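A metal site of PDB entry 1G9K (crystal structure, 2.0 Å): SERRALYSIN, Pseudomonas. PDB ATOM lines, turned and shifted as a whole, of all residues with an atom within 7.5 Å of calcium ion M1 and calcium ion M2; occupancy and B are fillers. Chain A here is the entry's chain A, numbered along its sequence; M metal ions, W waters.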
ATOM      1  N   LEU A 302      -2.250 -23.793 -17.285  1.00  0.00           N
ATOM      2  CA  LEU A 302      -3.321 -24.406 -18.062  1.00  0.00           C
ATOM      3  C   LEU A 302      -2.798 -25.266 -19.215  1.00  0.00           C
ATOM      4  O   LEU A 302      -3.577 -25.709 -20.054  1.00  0.00           O
ATOM      5  CB  LEU A 302      -4.274 -23.322 -18.606  1.00  0.00           C
ATOM      6  CG  LEU A 302      -5.056 -22.521 -17.557  1.00  0.00           C
ATOM      7  CD1 LEU A 302      -6.006 -21.534 -18.246  1.00  0.00           C
ATOM      8  CD2 LEU A 302      -5.845 -23.478 -16.677  1.00  0.00           C
ATOM      9  N   GLU A 326      -9.832 -23.971 -20.513  1.00  0.00           N
ATOM     10  CA  GLU A 326      -9.838 -22.574 -20.938  1.00  0.00           C
ATOM     11  C   GLU A 326      -9.602 -21.466 -19.918  1.00  0.00           C
ATOM     12  O   GLU A 326      -8.887 -20.495 -20.199  1.00  0.00           O
ATOM     13  CB  GLU A 326     -11.165 -22.268 -21.657  1.00  0.00           C
ATOM     14  CG  GLU A 326     -11.395 -23.017 -22.966  1.00  0.00           C
ATOM     15  CD  GLU A 326     -11.576 -24.513 -22.799  1.00  0.00           C
ATOM     16  OE1 GLU A 326     -12.057 -24.969 -21.740  1.00  0.00           O
ATOM     17  OE2 GLU A 326     -11.235 -25.251 -23.746  1.00  0.00           O
ATOM     18  N   ILE A 338      -0.674 -19.076 -15.885  1.00  0.00           N
ATOM     19  CA  ILE A 338      -0.162 -19.325 -17.226  1.00  0.00           C
ATOM     20  C   ILE A 338      -1.260 -19.955 -18.072  1.00  0.00           C
ATOM     21  O   ILE A 338      -1.774 -21.029 -17.753  1.00  0.00           O
ATOM     22  CB  ILE A 338       1.036 -20.281 -17.187  1.00  0.00           C
ATOM     23  CG1 ILE A 338       2.116 -19.704 -16.265  1.00  0.00           C
ATOM     24  CG2 ILE A 338       1.594 -20.483 -18.591  1.00  0.00           C
ATOM     25  CD1 ILE A 338       3.326 -20.589 -16.102  1.00  0.00           C
ATOM     26  N   GLY A 339      -1.621 -19.266 -19.150  1.00  0.00           N
ATOM     27  CA  GLY A 339      -2.658 -19.781 -20.037  1.00  0.00           C
ATOM     28  C   GLY A 339      -2.032 -20.671 -21.089  1.00  0.00           C
ATOM     29  O   GLY A 339      -0.846 -20.996 -21.010  1.00  0.00           O
ATOM     30  N   ASN A 340      -2.834 -21.059 -22.075  1.00  0.00           N
ATOM     31  CA  ASN A 340      -2.349 -21.903 -23.157  1.00  0.00           C
ATOM     32  C   ASN A 340      -2.639 -21.239 -24.511  1.00  0.00           C
ATOM     33  O   ASN A 340      -2.982 -20.054 -24.564  1.00  0.00           O
ATOM     34  CB  ASN A 340      -3.017 -23.279 -23.092  1.00  0.00           C
ATOM     35  CG  ASN A 340      -4.510 -23.204 -22.859  1.00  0.00           C
ATOM     36  OD1 ASN A 340      -5.209 -22.391 -23.468  1.00  0.00           O
ATOM     37  ND2 ASN A 340      -5.016 -24.061 -21.970  1.00  0.00           N
ATOM     38  N   ASP A 341      -2.513 -22.008 -25.585  1.00  0.00           N
ATOM     39  CA  ASP A 341      -2.741 -21.503 -26.946  1.00  0.00           C
ATOM     40  C   ASP A 341      -4.176 -21.086 -27.217  1.00  0.00           C
ATOM     41  O   ASP A 341      -4.442 -20.376 -28.198  1.00  0.00           O
ATOM     42  CB  ASP A 341      -2.336 -22.570 -27.968  1.00  0.00           C
ATOM     43  CG  ASP A 341      -0.842 -22.786 -28.029  1.00  0.00           C
ATOM     44  OD1 ASP A 341      -0.404 -23.751 -28.696  1.00  0.00           O
ATOM     45  OD2 ASP A 341      -0.110 -21.983 -27.406  1.00  0.00           O
ATOM     46  N   ALA A 342      -5.101 -21.513 -26.375  1.00  0.00           N
ATOM     47  CA  ALA A 342      -6.494 -21.157 -26.574  1.00  0.00           C
ATOM     48  C   ALA A 342      -6.810 -19.811 -25.940  1.00  0.00           C
ATOM     49  O   ALA A 342      -5.998 -19.264 -25.187  1.00  0.00           O
ATOM     50  CB  ALA A 342      -7.389 -22.246 -25.998  1.00  0.00           C
ATOM     51  N   ALA A 343      -7.981 -19.280 -26.271  1.00  0.00           N
ATOM     52  CA  ALA A 343      -8.425 -18.012 -25.709  1.00  0.00           C
ATOM     53  C   ALA A 343      -8.823 -18.307 -24.268  1.00  0.00           C
ATOM     54  O   ALA A 343      -9.772 -19.053 -24.027  1.00  0.00           O
ATOM     55  CB  ALA A 343      -9.625 -17.484 -26.489  1.00  0.00           C
ATOM     56  N   ASN A 344      -8.094 -17.720 -23.330  1.00  0.00           N
ATOM     57  CA  ASN A 344      -8.340 -17.963 -21.909  1.00  0.00           C
ATOM     58  C   ASN A 344      -8.884 -16.750 -21.170  1.00  0.00           C
ATOM     59  O   ASN A 344      -8.658 -15.610 -21.563  1.00  0.00           O
ATOM     60  CB  ASN A 344      -7.046 -18.365 -21.197  1.00  0.00           C
ATOM     61  CG  ASN A 344      -6.237 -19.393 -21.957  1.00  0.00           C
ATOM     62  OD1 ASN A 344      -5.065 -19.150 -22.279  1.00  0.00           O
ATOM     63  ND2 ASN A 344      -6.831 -20.549 -22.242  1.00  0.00           N
ATOM     64  N   VAL A 345      -9.608 -17.013 -20.085  1.00  0.00           N
ATOM     65  CA  VAL A 345     -10.104 -15.943 -19.227  1.00  0.00           C
ATOM     66  C   VAL A 345      -9.303 -16.204 -17.952  1.00  0.00           C
ATOM     67  O   VAL A 345      -9.465 -17.245 -17.320  1.00  0.00           O
ATOM     68  CB  VAL A 345     -11.603 -16.087 -18.927  1.00  0.00           C
ATOM     69  CG1 VAL A 345     -12.017 -15.040 -17.895  1.00  0.00           C
ATOM     70  CG2 VAL A 345     -12.424 -15.896 -20.203  1.00  0.00           C
ATOM     71  N   LEU A 346      -8.415 -15.278 -17.594  1.00  0.00           N
ATOM     72  CA  LEU A 346      -7.587 -15.433 -16.397  1.00  0.00           C
ATOM     73  C   LEU A 346      -7.825 -14.312 -15.394  1.00  0.00           C
ATOM     74  O   LEU A 346      -7.669 -13.128 -15.711  1.00  0.00           O
ATOM     75  CB  LEU A 346      -6.111 -15.451 -16.798  1.00  0.00           C
ATOM     76  CG  LEU A 346      -5.704 -16.445 -17.898  1.00  0.00           C
ATOM     77  CD1 LEU A 346      -4.256 -16.213 -18.322  1.00  0.00           C
ATOM     78  CD2 LEU A 346      -5.881 -17.871 -17.367  1.00  0.00           C
ATOM     79  N   TYR A 356      -0.008 -14.576 -17.612  1.00  0.00           N
ATOM     80  CA  TYR A 356       0.546 -14.841 -18.928  1.00  0.00           C
ATOM     81  C   TYR A 356      -0.537 -15.491 -19.772  1.00  0.00           C
ATOM     82  O   TYR A 356      -0.867 -16.660 -19.572  1.00  0.00           O
ATOM     83  CB  TYR A 356       1.716 -15.814 -18.791  1.00  0.00           C
ATOM     84  CG  TYR A 356       2.597 -15.916 -20.012  1.00  0.00           C
ATOM     85  CD1 TYR A 356       3.661 -15.034 -20.203  1.00  0.00           C
ATOM     86  CD2 TYR A 356       2.385 -16.911 -20.971  1.00  0.00           C
ATOM     87  CE1 TYR A 356       4.493 -15.135 -21.306  1.00  0.00           C
ATOM     88  CE2 TYR A 356       3.219 -17.023 -22.084  1.00  0.00           C
ATOM     89  CZ  TYR A 356       4.269 -16.131 -22.236  1.00  0.00           C
ATOM     90  OH  TYR A 356       5.116 -16.255 -23.323  1.00  0.00           O
ATOM     91  N   GLY A 357      -1.101 -14.735 -20.715  1.00  0.00           N
ATOM     92  CA  GLY A 357      -2.148 -15.266 -21.555  1.00  0.00           C
ATOM     93  C   GLY A 357      -1.695 -16.258 -22.619  1.00  0.00           C
ATOM     94  O   GLY A 357      -2.430 -17.188 -22.960  1.00  0.00           O
ATOM     95  N   GLY A 358      -0.488 -16.085 -23.132  1.00  0.00           N
ATOM     96  CA  GLY A 358      -0.003 -16.974 -24.167  1.00  0.00           C
ATOM     97  C   GLY A 358      -0.704 -16.708 -25.493  1.00  0.00           C
ATOM     98  O   GLY A 358      -1.236 -15.620 -25.703  1.00  0.00           O
ATOM     99  N   GLY A 359      -0.707 -17.704 -26.376  1.00  0.00           N
ATOM    100  CA  GLY A 359      -1.354 -17.545 -27.662  1.00  0.00           C
ATOM    101  C   GLY A 359      -2.848 -17.290 -27.570  1.00  0.00           C
ATOM    102  O   GLY A 359      -3.458 -17.526 -26.518  1.00  0.00           O
ATOM    103  N   GLY A 360      -3.442 -16.809 -28.662  1.00  0.00           N
ATOM    104  CA  GLY A 360      -4.861 -16.535 -28.683  1.00  0.00           C
ATOM    105  C   GLY A 360      -5.255 -15.219 -28.040  1.00  0.00           C
ATOM    106  O   GLY A 360      -4.441 -14.588 -27.355  1.00  0.00           O
ATOM    107  N   ALA A 361      -6.499 -14.798 -28.263  1.00  0.00           N
ATOM    108  CA  ALA A 361      -7.010 -13.553 -27.699  1.00  0.00           C
ATOM    109  C   ALA A 361      -7.558 -13.848 -26.312  1.00  0.00           C
ATOM    110  O   ALA A 361      -8.636 -14.412 -26.173  1.00  0.00           O
ATOM    111  CB  ALA A 361      -8.103 -12.988 -28.596  1.00  0.00           C
ATOM    112  N   ASP A 362      -6.805 -13.441 -25.293  1.00  0.00           N
ATOM    113  CA  ASP A 362      -7.195 -13.703 -23.916  1.00  0.00           C
ATOM    114  C   ASP A 362      -7.880 -12.518 -23.232  1.00  0.00           C
ATOM    115  O   ASP A 362      -7.655 -11.364 -23.578  1.00  0.00           O
ATOM    116  CB  ASP A 362      -5.963 -14.128 -23.107  1.00  0.00           C
ATOM    117  CG  ASP A 362      -5.243 -15.320 -23.735  1.00  0.00           C
ATOM    118  OD1 ASP A 362      -5.850 -16.402 -23.851  1.00  0.00           O
ATOM    119  OD2 ASP A 362      -4.059 -15.163 -24.121  1.00  0.00           O
ATOM    120  N   VAL A 363      -8.734 -12.840 -22.252  1.00  0.00           N
ATOM    121  CA  VAL A 363      -9.441 -11.837 -21.470  1.00  0.00           C
ATOM    122  C   VAL A 363      -8.790 -11.911 -20.107  1.00  0.00           C
ATOM    123  O   VAL A 363      -8.893 -12.916 -19.410  1.00  0.00           O
ATOM    124  CB  VAL A 363     -10.937 -12.164 -21.349  1.00  0.00           C
ATOM    125  CG1 VAL A 363     -11.646 -11.063 -20.589  1.00  0.00           C
ATOM    126  CG2 VAL A 363     -11.534 -12.357 -22.730  1.00  0.00           C
ATOM    127  N   LEU A 364      -8.097 -10.839 -19.727  1.00  0.00           N
ATOM    128  CA  LEU A 364      -7.370 -10.816 -18.466  1.00  0.00           C
ATOM    129  C   LEU A 364      -7.982  -9.900 -17.409  1.00  0.00           C
ATOM    130  O   LEU A 364      -8.378  -8.774 -17.700  1.00  0.00           O
ATOM    131  CB  LEU A 364      -5.927 -10.398 -18.725  1.00  0.00           C
ATOM    132  CG  LEU A 364      -5.229 -11.080 -19.906  1.00  0.00           C
ATOM    133  CD1 LEU A 364      -3.876 -10.431 -20.155  1.00  0.00           C
ATOM    134  CD2 LEU A 364      -5.064 -12.556 -19.610  1.00  0.00           C
ATOM    135  N   VAL A 374       2.259 -10.272 -18.412  1.00  0.00           N
ATOM    136  CA  VAL A 374       3.446 -10.610 -19.184  1.00  0.00           C
ATOM    137  C   VAL A 374       3.157 -11.131 -20.600  1.00  0.00           C
ATOM    138  O   VAL A 374       2.179 -11.842 -20.829  1.00  0.00           O
ATOM    139  CB  VAL A 374       4.296 -11.685 -18.426  1.00  0.00           C
ATOM    140  CG1 VAL A 374       5.571 -11.989 -19.199  1.00  0.00           C
ATOM    141  CG2 VAL A 374       4.617 -11.187 -17.030  1.00  0.00           C
ATOM    142  N   PHE A 375       4.031 -10.752 -21.524  1.00  0.00           N
ATOM    143  CA  PHE A 375       3.926 -11.168 -22.920  1.00  0.00           C
ATOM    144  C   PHE A 375       5.284 -11.724 -23.316  1.00  0.00           C
ATOM    145  O   PHE A 375       6.302 -11.053 -23.163  1.00  0.00           O
ATOM    146  CB  PHE A 375       3.544  -9.970 -23.797  1.00  0.00           C
ATOM    147  CG  PHE A 375       2.161  -9.476 -23.537  1.00  0.00           C
ATOM    148  CD1 PHE A 375       1.073 -10.018 -24.226  1.00  0.00           C
ATOM    149  CD2 PHE A 375       1.935  -8.518 -22.557  1.00  0.00           C
ATOM    150  CE1 PHE A 375      -0.216  -9.617 -23.924  1.00  0.00           C
ATOM    151  CE2 PHE A 375       0.634  -8.111 -22.253  1.00  0.00           C
ATOM    152  CZ  PHE A 375      -0.448  -8.657 -22.936  1.00  0.00           C
ATOM    153  N   ALA A 377       5.847 -13.322 -26.498  1.00  0.00           N
ATOM    154  CA  ALA A 377       6.008 -13.338 -27.947  1.00  0.00           C
ATOM    155  C   ALA A 377       5.010 -12.381 -28.591  1.00  0.00           C
ATOM    156  O   ALA A 377       3.936 -12.126 -28.035  1.00  0.00           O
ATOM    157  CB  ALA A 377       5.801 -14.751 -28.478  1.00  0.00           C
ATOM    158  N   SER A 379       3.253 -12.895 -31.138  1.00  0.00           N
ATOM    159  CA  SER A 379       2.066 -13.677 -31.481  1.00  0.00           C
ATOM    160  C   SER A 379       1.099 -13.832 -30.302  1.00  0.00           C
ATOM    161  O   SER A 379      -0.031 -14.287 -30.485  1.00  0.00           O
ATOM    162  CB  SER A 379       2.467 -15.061 -31.987  1.00  0.00           C
ATOM    163  OG  SER A 379       3.216 -15.760 -31.013  1.00  0.00           O
ATOM    164  N   ASP A 380       1.529 -13.465 -29.104  1.00  0.00           N
ATOM    165  CA  ASP A 380       0.666 -13.570 -27.930  1.00  0.00           C
ATOM    166  C   ASP A 380      -0.530 -12.625 -28.029  1.00  0.00           C
ATOM    167  O   ASP A 380      -1.617 -12.947 -27.545  1.00  0.00           O
ATOM    168  CB  ASP A 380       1.431 -13.240 -26.638  1.00  0.00           C
ATOM    169  CG  ASP A 380       2.323 -14.378 -26.170  1.00  0.00           C
ATOM    170  OD1 ASP A 380       2.409 -15.403 -26.873  1.00  0.00           O
ATOM    171  OD2 ASP A 380       2.948 -14.236 -25.106  1.00  0.00           O
ATOM    172  N   SER A 381      -0.331 -11.476 -28.667  1.00  0.00           N
ATOM    173  CA  SER A 381      -1.404 -10.487 -28.794  1.00  0.00           C
ATOM    174  C   SER A 381      -1.240  -9.655 -30.068  1.00  0.00           C
ATOM    175  O   SER A 381      -0.610  -8.607 -30.068  1.00  0.00           O
ATOM    176  CB  SER A 381      -1.399  -9.577 -27.568  1.00  0.00           C
ATOM    177  OG  SER A 381      -2.654  -8.949 -27.390  1.00  0.00           O
ATOM    178  N   THR A 382      -1.835 -10.143 -31.152  1.00  0.00           N
ATOM    179  CA  THR A 382      -1.768  -9.496 -32.450  1.00  0.00           C
ATOM    180  C   THR A 382      -3.034  -8.704 -32.742  1.00  0.00           C
ATOM    181  O   THR A 382      -4.063  -8.907 -32.095  1.00  0.00           O
ATOM    182  CB  THR A 382      -1.591 -10.549 -33.567  1.00  0.00           C
ATOM    183  OG1 THR A 382      -2.773 -11.358 -33.640  1.00  0.00           O
ATOM    184  CG2 THR A 382      -0.400 -11.441 -33.275  1.00  0.00           C
ATOM    185  N   ALA A 385      -6.021 -11.133 -33.204  1.00  0.00           N
ATOM    186  CA  ALA A 385      -6.488 -11.709 -31.940  1.00  0.00           C
ATOM    187  C   ALA A 385      -5.733 -11.080 -30.784  1.00  0.00           C
ATOM    188  O   ALA A 385      -4.774 -11.655 -30.263  1.00  0.00           O
ATOM    189  CB  ALA A 385      -6.268 -13.217 -31.957  1.00  0.00           C
ATOM    190  N   ALA A 386      -6.175  -9.899 -30.358  1.00  0.00           N
ATOM    191  CA  ALA A 386      -5.512  -9.183 -29.267  1.00  0.00           C
ATOM    192  C   ALA A 386      -6.142  -9.429 -27.905  1.00  0.00           C
ATOM    193  O   ALA A 386      -7.353  -9.619 -27.780  1.00  0.00           O
ATOM    194  CB  ALA A 386      -5.504  -7.693 -29.571  1.00  0.00           C
ATOM    195  N   ASP A 387      -5.304  -9.391 -26.882  1.00  0.00           N
ATOM    196  CA  ASP A 387      -5.722  -9.568 -25.508  1.00  0.00           C
ATOM    197  C   ASP A 387      -6.465  -8.327 -25.049  1.00  0.00           C
ATOM    198  O   ASP A 387      -6.386  -7.276 -25.684  1.00  0.00           O
ATOM    199  CB  ASP A 387      -4.508  -9.753 -24.593  1.00  0.00           C
ATOM    200  CG  ASP A 387      -3.981 -11.165 -24.579  1.00  0.00           C
ATOM    201  OD1 ASP A 387      -4.298 -11.952 -25.497  1.00  0.00           O
ATOM    202  OD2 ASP A 387      -3.242 -11.494 -23.638  1.00  0.00           O
ATOM    203  N   ILE A 388      -7.161  -8.451 -23.933  1.00  0.00           N
ATOM    204  CA  ILE A 388      -7.887  -7.335 -23.358  1.00  0.00           C
ATOM    205  C   ILE A 388      -7.827  -7.407 -21.831  1.00  0.00           C
ATOM    206  O   ILE A 388      -8.139  -8.452 -21.241  1.00  0.00           O
ATOM    207  CB  ILE A 388      -9.359  -7.319 -23.820  1.00  0.00           C
ATOM    208  CG1 ILE A 388     -10.109  -6.168 -23.142  1.00  0.00           C
ATOM    209  CG2 ILE A 388     -10.023  -8.657 -23.514  1.00  0.00           C
ATOM    210  CD1 ILE A 388     -11.535  -6.010 -23.624  1.00  0.00           C
HETATM  211 CA    CA M   1      -2.816 -13.879 -25.768  1.00  0.00          CA
HETATM  212 CA    CA M   2      -4.168 -18.032 -24.284  1.00  0.00          CA
HETATM  213  O   HOH W   1      -1.345 -13.071 -24.208  1.00  0.00           O
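N of Ala 377 sits at hydrogen-bond distance from OD2 of Asp 380.
The backbone NH (N) of Ile 388 sits at hydrogen-bond distance from the backbone carbonyl oxygen (O) of Asp 362.
The backbone NH of Asp 387 sits at hydrogen-bond distance from the side-chain hydroxyl of Ser 381 (2.7 Å).
The side-chain hydroxyl (OH) of Tyr 356 is in hydrogen-bond range of the side-chain carboxylate (OD2) of Asp 380.
N of Ala 342 sits at hydrogen-bond distance from OD1 of Asn 340, at 3.0 Å.
ND2 of Asn 344 lies within hydrogen-bond range of O of Glu 326, at 2.9 Å.
The side-chain amide nitrogen (ND2) of Asn 340 sits at hydrogen-bond distance from the backbone carbonyl oxygen (O) of Leu 302 (2.9 Å).
The backbone carbonyl oxygen (O) of Asn 344 lies within hydrogen-bond range of the backbone NH (N) of Val 363.
Within 4 Å of calcium ion M1: Gly 358, Gly 359, Gly 360, Asp 362, Asp 380 and Asp 387.
Calcium ion M1 is bound by water W1, the backbone carbonyl oxygen of Asp 380, the backbone carbonyl oxygen of Gly 358, the backbone carbonyl oxygen of Gly 360, the side-chain carboxylate of Asp 362 and the side-chain carboxylate of Asp 387.
Calcium ion M1 has six donor atoms within binding distance.
Calcium ion M2 is bound by the backbone carbonyl oxygen (O) of Gly 357 (2.3 Å), the backbone carbonyl oxygen (O) of Asn 340 (2.4 Å), the side-chain carboxylate (OD1) of Asp 362 (2.4 Å), the backbone carbonyl oxygen (O) of Ala 342 (2.4 Å), the backbone carbonyl oxygen (O) of Gly 359 (2.4 Å), the side-chain amide oxygen (OD1) of Asn 344 (2.5 Å) and the side-chain carboxylate (OD2) of Asp 362 (2.9 Å).
Calcium ion M2 has seven donor atoms within binding distance.
Water W1 bridges the side-chain carboxylate (OD2) of Asp 387 and the backbone NH (N) of Gly 358.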
